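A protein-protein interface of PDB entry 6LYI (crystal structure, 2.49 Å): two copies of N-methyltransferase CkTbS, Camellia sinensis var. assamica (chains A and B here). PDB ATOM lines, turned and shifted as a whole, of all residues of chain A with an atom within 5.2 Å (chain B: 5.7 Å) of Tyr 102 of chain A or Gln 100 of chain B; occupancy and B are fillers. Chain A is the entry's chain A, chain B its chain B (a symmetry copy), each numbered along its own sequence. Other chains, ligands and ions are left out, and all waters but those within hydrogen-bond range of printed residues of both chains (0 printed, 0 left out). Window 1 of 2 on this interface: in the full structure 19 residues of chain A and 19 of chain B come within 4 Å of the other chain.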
ATOM      1  N   ASN A  62      18.769  34.767 -18.292  1.00  0.00           N
ATOM      2  CA  ASN A  62      20.047  34.341 -18.825  1.00  0.00           C
ATOM      3  C   ASN A  62      20.773  35.483 -19.504  1.00  0.00           C
ATOM      4  O   ASN A  62      20.261  36.113 -20.427  1.00  0.00           O
ATOM      5  CB  ASN A  62      19.863  33.185 -19.791  1.00  0.00           C
ATOM      6  CG  ASN A  62      19.295  31.964 -19.118  1.00  0.00           C
ATOM      7  OD1 ASN A  62      19.545  31.727 -17.935  1.00  0.00           O
ATOM      8  ND2 ASN A  62      18.515  31.181 -19.860  1.00  0.00           N
ATOM      9  N   ALA A  63      21.971  35.750 -19.004  1.00  0.00           N
ATOM     10  CA  ALA A  63      22.812  36.822 -19.496  1.00  0.00           C
ATOM     11  C   ALA A  63      24.170  36.268 -19.910  1.00  0.00           C
ATOM     12  O   ALA A  63      24.721  35.406 -19.239  1.00  0.00           O
ATOM     13  CB  ALA A  63      22.971  37.893 -18.437  1.00  0.00           C
ATOM     14  N   ALA A  64      24.707  36.767 -21.014  1.00  0.00           N
ATOM     15  CA  ALA A  64      26.009  36.313 -21.493  1.00  0.00           C
ATOM     16  C   ALA A  64      26.984  37.475 -21.604  1.00  0.00           C
ATOM     17  O   ALA A  64      26.638  38.552 -22.089  1.00  0.00           O
ATOM     18  CB  ALA A  64      25.871  35.609 -22.827  1.00  0.00           C
ATOM     19  N   ASP A  65      28.194  37.257 -21.108  1.00  0.00           N
ATOM     20  CA  ASP A  65      29.294  38.181 -21.343  1.00  0.00           C
ATOM     21  C   ASP A  65      30.212  37.536 -22.379  1.00  0.00           C
ATOM     22  O   ASP A  65      30.803  36.489 -22.125  1.00  0.00           O
ATOM     23  CB  ASP A  65      30.057  38.493 -20.058  1.00  0.00           C
ATOM     24  CG  ASP A  65      30.865  39.780 -20.156  1.00  0.00           C
ATOM     25  OD1 ASP A  65      31.438  40.058 -21.226  1.00  0.00           O
ATOM     26  OD2 ASP A  65      30.915  40.526 -19.161  1.00  0.00           O
ATOM     27  N   GLN A 100      21.278  33.376 -14.310  1.00  0.00           N
ATOM     28  CA  GLN A 100      22.335  32.533 -14.848  1.00  0.00           C
ATOM     29  C   GLN A 100      23.229  33.360 -15.763  1.00  0.00           C
ATOM     30  O   GLN A 100      22.766  33.941 -16.742  1.00  0.00           O
ATOM     31  CB  GLN A 100      21.754  31.337 -15.605  1.00  0.00           C
ATOM     32  CG  GLN A 100      22.807  30.324 -16.064  1.00  0.00           C
ATOM     33  CD  GLN A 100      22.194  29.140 -16.788  1.00  0.00           C
ATOM     34  OE1 GLN A 100      22.867  28.450 -17.556  1.00  0.00           O
ATOM     35  NE2 GLN A 100      20.905  28.897 -16.549  1.00  0.00           N
ATOM     36  N   VAL A 101      24.511  33.421 -15.434  1.00  0.00           N
ATOM     37  CA  VAL A 101      25.459  34.176 -16.239  1.00  0.00           C
ATOM     38  C   VAL A 101      26.408  33.255 -17.012  1.00  0.00           C
ATOM     39  O   VAL A 101      27.022  32.348 -16.442  1.00  0.00           O
ATOM     40  CB  VAL A 101      26.277  35.138 -15.369  1.00  0.00           C
ATOM     41  CG1 VAL A 101      27.392  35.788 -16.191  1.00  0.00           C
ATOM     42  CG2 VAL A 101      25.355  36.199 -14.751  1.00  0.00           C
ATOM     43  N   TYR A 102      26.508  33.480 -18.317  1.00  0.00           N
ATOM     44  CA  TYR A 102      27.451  32.753 -19.156  1.00  0.00           C
ATOM     45  C   TYR A 102      28.682  33.591 -19.461  1.00  0.00           C
ATOM     46  O   TYR A 102      28.562  34.698 -19.983  1.00  0.00           O
ATOM     47  CB  TYR A 102      26.808  32.345 -20.473  1.00  0.00           C
ATOM     48  CG  TYR A 102      25.666  31.364 -20.388  1.00  0.00           C
ATOM     49  CD1 TYR A 102      25.897  29.995 -20.372  1.00  0.00           C
ATOM     50  CD2 TYR A 102      24.354  31.804 -20.383  1.00  0.00           C
ATOM     51  CE1 TYR A 102      24.849  29.090 -20.323  1.00  0.00           C
ATOM     52  CE2 TYR A 102      23.306  30.914 -20.340  1.00  0.00           C
ATOM     53  CZ  TYR A 102      23.557  29.559 -20.308  1.00  0.00           C
ATOM     54  OH  TYR A 102      22.504  28.672 -20.264  1.00  0.00           O
ATOM     55  N   LEU A 103      29.848  33.048 -19.199  1.00  0.00           N
ATOM     56  CA  LEU A 103      31.056  33.771 -19.502  1.00  0.00           C
ATOM     57  C   LEU A 103      31.899  33.129 -20.580  1.00  0.00           C
ATOM     58  O   LEU A 103      32.462  32.084 -20.390  1.00  0.00           O
ATOM     59  CB  LEU A 103      31.908  33.942 -18.260  1.00  0.00           C
ATOM     60  CG  LEU A 103      31.331  34.615 -17.034  1.00  0.00           C
ATOM     61  CD1 LEU A 103      32.377  34.675 -15.960  1.00  0.00           C
ATOM     62  CD2 LEU A 103      30.851  36.002 -17.349  1.00  0.00           C
ATOM     63  N   ASN A 104      31.960  33.783 -21.722  1.00  0.00           N
ATOM     64  CA  ASN A 104      32.826  33.407 -22.828  1.00  0.00           C
ATOM     65  C   ASN A 104      34.079  34.263 -22.801  1.00  0.00           C
ATOM     66  O   ASN A 104      34.002  35.471 -23.006  1.00  0.00           O
ATOM     67  CB  ASN A 104      32.089  33.568 -24.160  1.00  0.00           C
ATOM     68  CG  ASN A 104      32.995  33.374 -25.353  1.00  0.00           C
ATOM     69  OD1 ASN A 104      33.505  34.340 -25.927  1.00  0.00           O
ATOM     70  ND2 ASN A 104      33.208  32.122 -25.733  1.00  0.00           N
ATOM     71  N   MET A 135      28.564  30.501 -15.294  1.00  0.00           N
ATOM     72  CA  MET A 135      28.990  29.394 -16.143  1.00  0.00           C
ATOM     73  C   MET A 135      30.062  29.822 -17.165  1.00  0.00           C
ATOM     74  O   MET A 135      30.025  30.934 -17.695  1.00  0.00           O
ATOM     75  CB  MET A 135      27.772  28.810 -16.869  1.00  0.00           C
ATOM     76  CG  MET A 135      27.386  27.414 -16.429  1.00  0.00           C
ATOM     77  SD  MET A 135      25.868  27.356 -15.485  1.00  0.00           S
ATOM     78  CE  MET A 135      26.437  27.763 -13.847  1.00  0.00           C
ATOM     79  N   VAL A 137      31.744  29.501 -20.863  1.00  0.00           N
ATOM     80  CA  VAL A 137      31.425  29.093 -22.233  1.00  0.00           C
ATOM     81  C   VAL A 137      32.633  29.195 -23.176  1.00  0.00           C
ATOM     82  O   VAL A 137      32.965  30.276 -23.662  1.00  0.00           O
ATOM     83  CB  VAL A 137      30.281  29.938 -22.818  1.00  0.00           C
ATOM     84  CG1 VAL A 137      29.872  29.402 -24.210  1.00  0.00           C
ATOM     85  CG2 VAL A 137      29.099  29.964 -21.871  1.00  0.00           C
ATOM     86  N   PHE A 146      25.045  29.159 -27.903  1.00  0.00           N
ATOM     87  CA  PHE A 146      23.895  28.875 -27.045  1.00  0.00           C
ATOM     88  C   PHE A 146      22.729  28.294 -27.838  1.00  0.00           C
ATOM     89  O   PHE A 146      22.651  28.473 -29.054  1.00  0.00           O
ATOM     90  CB  PHE A 146      23.445  30.153 -26.316  1.00  0.00           C
ATOM     91  CG  PHE A 146      24.553  30.843 -25.574  1.00  0.00           C
ATOM     92  CD1 PHE A 146      24.973  30.376 -24.336  1.00  0.00           C
ATOM     93  CD2 PHE A 146      25.186  31.952 -26.117  1.00  0.00           C
ATOM     94  CE1 PHE A 146      26.008  31.001 -23.655  1.00  0.00           C
ATOM     95  CE2 PHE A 146      26.226  32.583 -25.436  1.00  0.00           C
ATOM     96  CZ  PHE A 146      26.641  32.103 -24.210  1.00  0.00           C
ATOM     97  N   PRO A 147      21.823  27.581 -27.152  1.00  0.00           N
ATOM     98  CA  PRO A 147      20.589  27.159 -27.822  1.00  0.00           C
ATOM     99  C   PRO A 147      19.761  28.356 -28.302  1.00  0.00           C
ATOM    100  O   PRO A 147      19.954  29.475 -27.829  1.00  0.00           O
ATOM    101  CB  PRO A 147      19.844  26.376 -26.728  1.00  0.00           C
ATOM    102  CG  PRO A 147      20.934  25.894 -25.810  1.00  0.00           C
ATOM    103  CD  PRO A 147      21.962  26.992 -25.806  1.00  0.00           C
ATOM    104  N   LEU A 151      18.863  33.561 -24.463  1.00  0.00           N
ATOM    105  CA  LEU A 151      19.472  34.728 -23.839  1.00  0.00           C
ATOM    106  C   LEU A 151      18.510  35.890 -23.740  1.00  0.00           C
ATOM    107  O   LEU A 151      17.840  36.241 -24.709  1.00  0.00           O
ATOM    108  CB  LEU A 151      20.716  35.161 -24.611  1.00  0.00           C
ATOM    109  CG  LEU A 151      21.834  34.136 -24.734  1.00  0.00           C
ATOM    110  CD1 LEU A 151      22.990  34.737 -25.517  1.00  0.00           C
ATOM    111  CD2 LEU A 151      22.285  33.674 -23.362  1.00  0.00           C
ATOM    112  N   ALA B  60      15.369  22.516 -26.495  1.00  0.00           N
ATOM    113  CA  ALA B  60      16.693  21.986 -26.178  1.00  0.00           C
ATOM    114  C   ALA B  60      16.638  20.979 -25.042  1.00  0.00           C
ATOM    115  O   ALA B  60      15.888  21.145 -24.086  1.00  0.00           O
ATOM    116  CB  ALA B  60      17.653  23.109 -25.818  1.00  0.00           C
ATOM    117  N   LEU B  61      17.444  19.934 -25.151  1.00  0.00           N
ATOM    118  CA  LEU B  61      17.670  19.022 -24.039  1.00  0.00           C
ATOM    119  C   LEU B  61      18.845  19.525 -23.194  1.00  0.00           C
ATOM    120  O   LEU B  61      19.900  19.870 -23.736  1.00  0.00           O
ATOM    121  CB  LEU B  61      17.946  17.615 -24.552  1.00  0.00           C
ATOM    122  CG  LEU B  61      17.869  16.531 -23.483  1.00  0.00           C
ATOM    123  CD1 LEU B  61      16.439  16.375 -22.983  1.00  0.00           C
ATOM    124  CD2 LEU B  61      18.406  15.226 -24.041  1.00  0.00           C
ATOM    125  N   ASN B  62      18.666  19.560 -21.877  1.00  0.00           N
ATOM    126  CA  ASN B  62      19.688  20.080 -20.965  1.00  0.00           C
ATOM    127  C   ASN B  62      20.293  19.009 -20.080  1.00  0.00           C
ATOM    128  O   ASN B  62      19.642  18.536 -19.143  1.00  0.00           O
ATOM    129  CB  ASN B  62      19.103  21.173 -20.073  1.00  0.00           C
ATOM    130  CG  ASN B  62      18.677  22.389 -20.851  1.00  0.00           C
ATOM    131  OD1 ASN B  62      19.177  22.649 -21.953  1.00  0.00           O
ATOM    132  ND2 ASN B  62      17.759  23.154 -20.281  1.00  0.00           N
ATOM    133  N   ALA B  63      21.532  18.632 -20.379  1.00  0.00           N
ATOM    134  CA  ALA B  63      22.211  17.564 -19.647  1.00  0.00           C
ATOM    135  C   ALA B  63      23.404  18.072 -18.831  1.00  0.00           C
ATOM    136  O   ALA B  63      24.126  18.970 -19.257  1.00  0.00           O
ATOM    137  CB  ALA B  63      22.664  16.464 -20.623  1.00  0.00           C
ATOM    138  N   ALA B  64      23.600  17.488 -17.651  1.00  0.00           N
ATOM    139  CA  ALA B  64      24.753  17.812 -16.823  1.00  0.00           C
ATOM    140  C   ALA B  64      25.542  16.557 -16.467  1.00  0.00           C
ATOM    141  O   ALA B  64      24.960  15.498 -16.189  1.00  0.00           O
ATOM    142  CB  ALA B  64      24.320  18.537 -15.553  1.00  0.00           C
ATOM    143  N   GLU B  98      18.252  21.144 -29.937  1.00  0.00           N
ATOM    144  CA  GLU B  98      19.661  21.254 -29.651  1.00  0.00           C
ATOM    145  C   GLU B  98      19.965  20.600 -28.304  1.00  0.00           C
ATOM    146  O   GLU B  98      19.063  20.240 -27.557  1.00  0.00           O
ATOM    147  CB  GLU B  98      20.068  22.721 -29.676  1.00  0.00           C
ATOM    148  CG  GLU B  98      19.623  23.418 -30.958  1.00  0.00           C
ATOM    149  CD  GLU B  98      19.761  24.930 -30.893  1.00  0.00           C
ATOM    150  OE1 GLU B  98      19.055  25.547 -30.065  1.00  0.00           O
ATOM    151  OE2 GLU B  98      20.571  25.506 -31.659  1.00  0.00           O
ATOM    152  N   LEU B  99      21.243  20.430 -28.019  1.00  0.00           N
ATOM    153  CA  LEU B  99      21.696  19.807 -26.788  1.00  0.00           C
ATOM    154  C   LEU B  99      22.621  20.758 -26.042  1.00  0.00           C
ATOM    155  O   LEU B  99      23.609  21.243 -26.613  1.00  0.00           O
ATOM    156  CB  LEU B  99      22.429  18.496 -27.088  1.00  0.00           C
ATOM    157  CG  LEU B  99      23.004  17.755 -25.885  1.00  0.00           C
ATOM    158  CD1 LEU B  99      21.877  17.287 -24.932  1.00  0.00           C
ATOM    159  CD2 LEU B  99      23.897  16.596 -26.334  1.00  0.00           C
ATOM    160  N   GLN B 100      22.296  21.046 -24.782  1.00  0.00           N
ATOM    161  CA  GLN B 100      23.167  21.859 -23.944  1.00  0.00           C
ATOM    162  C   GLN B 100      23.791  20.978 -22.866  1.00  0.00           C
ATOM    163  O   GLN B 100      23.100  20.336 -22.086  1.00  0.00           O
ATOM    164  CB  GLN B 100      22.409  23.031 -23.323  1.00  0.00           C
ATOM    165  CG  GLN B 100      23.292  23.970 -22.519  1.00  0.00           C
ATOM    166  CD  GLN B 100      22.512  25.148 -21.982  1.00  0.00           C
ATOM    167  OE1 GLN B 100      21.329  25.029 -21.677  1.00  0.00           O
ATOM    168  NE2 GLN B 100      23.166  26.293 -21.872  1.00  0.00           N
ATOM    169  N   VAL B 101      25.111  20.931 -22.853  1.00  0.00           N
ATOM    170  CA  VAL B 101      25.815  20.065 -21.937  1.00  0.00           C
ATOM    171  C   VAL B 101      26.553  20.886 -20.878  1.00  0.00           C
ATOM    172  O   VAL B 101      27.388  21.732 -21.203  1.00  0.00           O
ATOM    173  CB  VAL B 101      26.805  19.180 -22.690  1.00  0.00           C
ATOM    174  CG1 VAL B 101      27.546  18.319 -21.726  1.00  0.00           C
ATOM    175  CG2 VAL B 101      26.077  18.335 -23.718  1.00  0.00           C
ATOM    176  N   TYR B 102      26.230  20.645 -19.614  1.00  0.00           N
ATOM    177  CA  TYR B 102      26.941  21.278 -18.516  1.00  0.00           C
ATOM    178  C   TYR B 102      27.953  20.322 -17.898  1.00  0.00           C
ATOM    179  O   TYR B 102      27.570  19.253 -17.415  1.00  0.00           O
ATOM    180  CB  TYR B 102      25.969  21.729 -17.449  1.00  0.00           C
ATOM    181  CG  TYR B 102      24.948  22.770 -17.859  1.00  0.00           C
ATOM    182  CD1 TYR B 102      25.273  24.119 -17.885  1.00  0.00           C
ATOM    183  CD2 TYR B 102      23.635  22.409 -18.141  1.00  0.00           C
ATOM    184  CE1 TYR B 102      24.329  25.079 -18.209  1.00  0.00           C
ATOM    185  CE2 TYR B 102      22.682  23.361 -18.468  1.00  0.00           C
ATOM    186  CZ  TYR B 102      23.031  24.696 -18.499  1.00  0.00           C
ATOM    187  OH  TYR B 102      22.074  25.640 -18.827  1.00  0.00           O
ATOM    188  N   SER B 131      22.748  20.221 -32.732  1.00  0.00           N
ATOM    189  CA  SER B 131      23.841  21.064 -32.273  1.00  0.00           C
ATOM    190  C   SER B 131      24.114  20.773 -30.808  1.00  0.00           C
ATOM    191  O   SER B 131      23.190  20.536 -30.038  1.00  0.00           O
ATOM    192  CB  SER B 131      23.520  22.549 -32.463  1.00  0.00           C
ATOM    193  OG  SER B 131      23.258  22.877 -33.815  1.00  0.00           O
ATOM    194  N   CYS B 132      25.383  20.798 -30.428  1.00  0.00           N
ATOM    195  CA  CYS B 132      25.753  20.547 -29.056  1.00  0.00           C
ATOM    196  C   CYS B 132      26.563  21.725 -28.525  1.00  0.00           C
ATOM    197  O   CYS B 132      27.574  22.106 -29.100  1.00  0.00           O
ATOM    198  CB  CYS B 132      26.546  19.241 -28.941  1.00  0.00           C
ATOM    199  SG  CYS B 132      26.920  18.754 -27.282  1.00  0.00           S
ATOM    200  N   TYR B 133      26.099  22.295 -27.419  1.00  0.00           N
ATOM    201  CA  TYR B 133      26.738  23.442 -26.804  1.00  0.00           C
ATOM    202  C   TYR B 133      27.279  23.040 -25.445  1.00  0.00           C
ATOM    203  O   TYR B 133      26.526  22.622 -24.566  1.00  0.00           O
ATOM    204  CB  TYR B 133      25.743  24.594 -26.688  1.00  0.00           C
ATOM    205  CG  TYR B 133      25.109  24.956 -28.010  1.00  0.00           C
ATOM    206  CD1 TYR B 133      25.840  25.596 -28.999  1.00  0.00           C
ATOM    207  CD2 TYR B 133      23.782  24.649 -28.273  1.00  0.00           C
ATOM    208  CE1 TYR B 133      25.272  25.923 -30.210  1.00  0.00           C
ATOM    209  CE2 TYR B 133      23.200  24.978 -29.478  1.00  0.00           C
ATOM    210  CZ  TYR B 133      23.952  25.614 -30.449  1.00  0.00           C
ATOM    211  OH  TYR B 133      23.387  25.946 -31.667  1.00  0.00           O
ATOM    212  N   MET B 135      29.251  23.679 -21.908  1.00  0.00           N
ATOM    213  CA  MET B 135      29.591  24.673 -20.902  1.00  0.00           C
ATOM    214  C   MET B 135      30.340  24.064 -19.732  1.00  0.00           C
ATOM    215  O   MET B 135      30.193  22.875 -19.431  1.00  0.00           O
ATOM    216  CB  MET B 135      28.335  25.371 -20.361  1.00  0.00           C
ATOM    217  CG  MET B 135      27.909  26.593 -21.134  1.00  0.00           C
ATOM    218  SD  MET B 135      26.985  26.098 -22.559  1.00  0.00           S
ATOM    219  CE  MET B 135      26.489  27.660 -23.206  1.00  0.00           C
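Tyr 102 of chain A touches just these residues of chain B: Gln 100, Tyr 102 and Met 135.
Of the printed residues of chain B, Met 135 of chain A touches Tyr 102 (3.9 Å).
Printed residues of chain B within 4 Å of Val 137 of chain A: Met 135.
Of the printed residues of chain B, Pro 147 of chain A touches Glu 98 (3.2 Å) and Tyr 133 (3.7 Å).
Of the printed residues of chain A, Gln 100 of chain B touches Tyr 102.
Of the printed residues of chain A, Tyr 102 of chain B touches Gln 100 (3.2 Å), Tyr 102 (3.4 Å) and Met 135 (3.9 Å).
Of the printed residues of chain A, Met 135 of chain B touches Tyr 102 (3.6 Å), Val 137 (3.7 Å) and Phe 146 (3.3 Å).
The nearest printed residue of chain B that does not touch Tyr 102 of chain A is Asn 62 of chain B (7.1 Å).
OE2 of Glu 98 of chain B is in hydrogen-bond range of OH of Tyr 133 of chain B (2.9 Å).
N of Val 101 of chain B is in hydrogen-bond range of O of Tyr 133 of chain B (2.8 Å).
The backbone carbonyl oxygen of Val 101 of chain A is in hydrogen-bond range of the backbone NH of Met 135 of chain A, at 2.7 Å.
N of Val 137 of chain A is in hydrogen-bond range of O of Leu 103 of chain A, at 2.7 Å.
N of Leu 103 of chain A lies within hydrogen-bond range of O of Met 135 of chain A (2.6 Å).
The backbone carbonyl oxygen (O) of Val 101 of chain B is in hydrogen-bond range of the backbone NH (N) of Met 135 of chain B (2.8 Å).
CE1 of Tyr 102 of chain A touches CE of Met 135 of chain B (3.6 Å).
Tyr 102 of chain B touches Met 135 of chain A (CE1 to SD, 3.9 Å).
Val 137 of chain A touches Met 135 of chain B (CG2 to CG, 3.7 Å).
O of Phe 146 of chain A touches CZ of Tyr 133 of chain B, at 3.4 Å.
Phe 146 of chain A touches Met 135 of chain B (CD1 to CE, 3.3 Å).
Glu 98 of chain B touches Pro 147 of chain A.
Tyr 133 of chain B touches Pro 147 of chain A (CD2 to N, 3.7 Å).
Gln 100 of chain A touches Tyr 102 of chain B, and with the chains exchanged Tyr 102 of chain A touches Gln 100 of chain B.
Tyr 102 of chain A touches its own counterpart, Tyr 102 of chain B.
Tyr 102 of chain A touches Met 135 of chain B, and with the chains exchanged Met 135 of chain A touches Tyr 102 of chain B.
Of the 14 printed residues of chain B, 5 touch a printed residue of chain A.
Printed residues of chain A that touch a printed residue of chain B: Gln 100, Tyr 102, Met 135, Val 137, Phe 146 and Pro 147.
Hydrophobic or aromatic side chains of chain A that line the printed part of chain B: Tyr 102, Met 135, Val 137, Phe 146 and Pro 147.
Among the printed residues, 10 pairs touch across the chains.
The side-chain amide nitrogen (NE2) of Gln 100 of chain B is in hydrogen-bond range of the side-chain hydroxyl (OH) of Tyr 102 of chain A (2.9 Å).
OH of Tyr 102 of chain B sits at hydrogen-bond distance from OH of Tyr 102 of chain A.
The side-chain amide oxygen of Gln 100 of chain A lies within hydrogen-bond range of the side-chain hydroxyl of Tyr 102 of chain B (3.2 Å).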
